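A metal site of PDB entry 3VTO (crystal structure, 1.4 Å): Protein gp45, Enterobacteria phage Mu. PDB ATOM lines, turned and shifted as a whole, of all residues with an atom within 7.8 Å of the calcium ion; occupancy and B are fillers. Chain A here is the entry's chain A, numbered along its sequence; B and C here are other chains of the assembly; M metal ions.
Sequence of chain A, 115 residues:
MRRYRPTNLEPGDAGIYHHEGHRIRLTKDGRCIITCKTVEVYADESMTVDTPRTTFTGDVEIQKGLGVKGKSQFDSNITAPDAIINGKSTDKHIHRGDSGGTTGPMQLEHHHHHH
The backbone NH (N) of Gly 100 of chain A is in hydrogen-bond range of the side-chain carboxylate (OD2) of Asp 98 of chain C (3.1 Å).
The backbone NH (N) of Gly 101 of chain A sits at hydrogen-bond distance from the side-chain carboxylate (OD2) of Asp 98 of chain C (2.9 Å).
The side-chain carboxylate (OD2) of Asp 98 of chain A sits at hydrogen-bond distance from the backbone NH (N) of Gly 101 of chain B.
N of Gly 101 of chain C lies within hydrogen-bond range of OD2 of Asp 98 of chain B.
The side-chain carboxylate of Asp 98 of chain A lies within hydrogen-bond range of the backbone NH of Gly 100 of chain B (3.1 Å).
OD2 of Asp 98 of chain B sits at hydrogen-bond distance from N of Gly 100 of chain C (3.3 Å).
The nearest printed residue that does not touch the calcium ion is Gly 97 of chain B (5.3 Å).
OD1 of Asp 98 of chain B binds the calcium ion.
The calcium ion is bound by OD1 of Asp 98 of chain A (2.2 Å).
The side-chain carboxylate (OD1) of Asp 98 of chain C is bound to the calcium ion.
OG of Ser 99 of chain C binds the calcium ion, 2.4 Å away.
OG of Ser 99 of chain A is bound to the calcium ion.
OG of Ser 99 of chain B binds the calcium ion (2.5 Å).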
ATOM      1  N   GLY A  97     -18.873  25.674  18.230  1.00  0.00           N
ATOM      2  CA  GLY A  97     -19.688  24.527  18.711  1.00  0.00           C
ATOM      3  C   GLY A  97     -18.872  23.580  19.581  1.00  0.00           C
ATOM      4  O   GLY A  97     -17.648  23.719  19.700  1.00  0.00           O
ATOM      5  N   ASP A  98     -19.546  22.602  20.191  1.00  0.00           N
ATOM      6  CA  ASP A  98     -18.854  21.704  21.134  1.00  0.00           C
ATOM      7  C   ASP A  98     -17.973  20.658  20.471  1.00  0.00           C
ATOM      8  O   ASP A  98     -17.329  19.877  21.179  1.00  0.00           O
ATOM      9  CB  ASP A  98     -19.853  21.072  22.139  1.00  0.00           C
ATOM     10  CG  ASP A  98     -20.818  20.078  21.511  1.00  0.00           C
ATOM     11  OD1 ASP A  98     -20.717  19.780  20.298  1.00  0.00           O
ATOM     12  OD2 ASP A  98     -21.649  19.579  22.261  1.00  0.00           O
ATOM     13  N   SER A  99     -17.928  20.671  19.145  1.00  0.00           N
ATOM     14  CA  SER A  99     -17.080  19.727  18.398  1.00  0.00           C
ATOM     15  C   SER A  99     -16.004  20.496  17.603  1.00  0.00           C
ATOM     16  O   SER A  99     -15.337  19.918  16.735  1.00  0.00           O
ATOM     17  CB  SER A  99     -17.889  18.863  17.463  1.00  0.00           C
ATOM     18  OG  SER A  99     -18.969  18.234  18.123  1.00  0.00           O
ATOM     19  N   GLY A 100     -15.896  21.800  17.837  1.00  0.00           N
ATOM     20  CA  GLY A 100     -14.878  22.639  17.205  1.00  0.00           C
ATOM     21  C   GLY A 100     -15.271  23.293  15.897  1.00  0.00           C
ATOM     22  O   GLY A 100     -14.446  23.936  15.269  1.00  0.00           O
ATOM     23  N   GLY A 101     -16.514  23.092  15.476  1.00  0.00           N
ATOM     24  CA  GLY A 101     -17.058  23.787  14.307  1.00  0.00           C
ATOM     25  C   GLY A 101     -17.773  25.043  14.751  1.00  0.00           C
ATOM     26  O   GLY A 101     -17.409  25.645  15.759  1.00  0.00           O
ATOM     27  N   THR A 103     -21.682  26.985  15.357  1.00  0.00           N
ATOM     28  CA  THR A 103     -23.121  26.836  15.393  1.00  0.00           C
ATOM     29  C   THR A 103     -23.767  27.734  14.341  1.00  0.00           C
ATOM     30  O   THR A 103     -23.131  28.571  13.709  1.00  0.00           O
ATOM     31  CB  THR A 103     -23.677  27.271  16.773  1.00  0.00           C
ATOM     32  OG1 THR A 103     -23.557  28.696  16.940  1.00  0.00           O
ATOM     33  CG2 THR A 103     -22.988  26.584  17.924  1.00  0.00           C
ATOM     34  N   GLY B  97     -23.740  22.146  23.855  1.00  0.00           N
ATOM     35  CA  GLY B  97     -23.765  21.891  22.414  1.00  0.00           C
ATOM     36  C   GLY B  97     -24.547  20.634  22.033  1.00  0.00           C
ATOM     37  O   GLY B  97     -25.018  19.886  22.913  1.00  0.00           O
ATOM     38  N   ASP B  98     -24.604  20.355  20.729  1.00  0.00           N
ATOM     39  CA  ASP B  98     -25.411  19.228  20.240  1.00  0.00           C
ATOM     40  C   ASP B  98     -24.783  17.857  20.503  1.00  0.00           C
ATOM     41  O   ASP B  98     -25.418  16.855  20.301  1.00  0.00           O
ATOM     42  CB  ASP B  98     -25.833  19.356  18.797  1.00  0.00           C
ATOM     43  CG  ASP B  98     -24.653  19.372  17.799  1.00  0.00           C
ATOM     44  OD1 ASP B  98     -23.414  19.175  18.156  1.00  0.00           O
ATOM     45  OD2 ASP B  98     -25.005  19.674  16.635  1.00  0.00           O
ATOM     46  N   SER B  99     -23.536  17.844  20.951  1.00  0.00           N
ATOM     47  CA  SER B  99     -22.831  16.617  21.332  1.00  0.00           C
ATOM     48  C   SER B  99     -22.631  16.501  22.862  1.00  0.00           C
ATOM     49  O   SER B  99     -21.866  15.638  23.336  1.00  0.00           O
ATOM     50  CB  SER B  99     -21.488  16.540  20.595  1.00  0.00           C
ATOM     51  OG  SER B  99     -21.611  16.828  19.200  1.00  0.00           O
ATOM     52  N   GLY B 100     -23.323  17.345  23.620  1.00  0.00           N
ATOM     53  CA  GLY B 100     -23.286  17.268  25.063  1.00  0.00           C
ATOM     54  C   GLY B 100     -22.103  17.907  25.746  1.00  0.00           C
ATOM     55  O   GLY B 100     -21.988  17.797  26.963  1.00  0.00           O
ATOM     56  N   GLY B 101     -21.276  18.620  24.970  1.00  0.00           N
ATOM     57  CA  GLY B 101     -20.222  19.438  25.536  1.00  0.00           C
ATOM     58  C   GLY B 101     -20.713  20.865  25.706  1.00  0.00           C
ATOM     59  O   GLY B 101     -21.899  21.128  25.788  1.00  0.00           O
ATOM     60  N   THR B 103     -20.388  24.911  24.170  1.00  0.00           N
ATOM     61  CA  THR B 103     -19.939  25.800  23.133  1.00  0.00           C
ATOM     62  C   THR B 103     -18.949  26.796  23.722  1.00  0.00           C
ATOM     63  O   THR B 103     -18.871  26.978  24.956  1.00  0.00           O
ATOM     64  CB  THR B 103     -21.083  26.571  22.475  1.00  0.00           C
ATOM     65  OG1 THR B 103     -21.606  27.534  23.385  1.00  0.00           O
ATOM     66  CG2 THR B 103     -22.173  25.632  22.003  1.00  0.00           C
ATOM     67  N   GLY C  97     -26.492  23.291  16.275  1.00  0.00           N
ATOM     68  CA  GLY C  97     -25.129  22.950  16.724  1.00  0.00           C
ATOM     69  C   GLY C  97     -24.184  22.674  15.573  1.00  0.00           C
ATOM     70  O   GLY C  97     -24.582  22.738  14.386  1.00  0.00           O
ATOM     71  N   ASP C  98     -22.915  22.405  15.907  1.00  0.00           N
ATOM     72  CA  ASP C  98     -21.942  22.165  14.879  1.00  0.00           C
ATOM     73  C   ASP C  98     -21.946  20.756  14.344  1.00  0.00           C
ATOM     74  O   ASP C  98     -21.133  20.460  13.456  1.00  0.00           O
ATOM     75  CB  ASP C  98     -20.519  22.620  15.306  1.00  0.00           C
ATOM     76  CG  ASP C  98     -19.944  21.801  16.451  1.00  0.00           C
ATOM     77  OD1 ASP C  98     -20.577  20.820  16.910  1.00  0.00           O
ATOM     78  OD2 ASP C  98     -18.811  22.120  16.878  1.00  0.00           O
ATOM     79  N   SER C  99     -22.885  19.899  14.794  1.00  0.00           N
ATOM     80  CA  SER C  99     -22.866  18.505  14.377  1.00  0.00           C
ATOM     81  C   SER C  99     -24.248  18.095  13.880  1.00  0.00           C
ATOM     82  O   SER C  99     -24.593  16.920  13.973  1.00  0.00           O
ATOM     83  CB  SER C  99     -22.498  17.549  15.527  1.00  0.00           C
ATOM     84  OG  SER C  99     -21.267  17.932  16.129  1.00  0.00           O
ATOM     85  N   GLY C 100     -25.025  19.037  13.360  1.00  0.00           N
ATOM     86  CA  GLY C 100     -26.323  18.663  12.786  1.00  0.00           C
ATOM     87  C   GLY C 100     -27.476  18.544  13.754  1.00  0.00           C
ATOM     88  O   GLY C 100     -28.602  18.180  13.350  1.00  0.00           O
ATOM     89  N   GLY C 101     -27.209  18.870  15.034  1.00  0.00           N
ATOM     90  CA  GLY C 101     -28.267  18.847  16.061  1.00  0.00           C
ATOM     91  C   GLY C 101     -28.611  20.251  16.494  1.00  0.00           C
ATOM     92  O   GLY C 101     -28.447  21.193  15.733  1.00  0.00           O
ATOM     93  N   THR C 103     -28.375  23.077  20.014  1.00  0.00           N
ATOM     94  CA  THR C 103     -27.805  23.327  21.323  1.00  0.00           C
ATOM     95  C   THR C 103     -28.924  23.476  22.361  1.00  0.00           C
ATOM     96  O   THR C 103     -30.119  23.584  21.979  1.00  0.00           O
ATOM     97  CB  THR C 103     -26.982  24.650  21.353  1.00  0.00           C
ATOM     98  OG1 THR C 103     -27.888  25.777  21.343  1.00  0.00           O
ATOM     99  CG2 THR C 103     -25.998  24.737  20.221  1.00  0.00           C
HETATM  100 CA    CA M   1     -21.260  19.061  18.245  1.00  0.00          CA
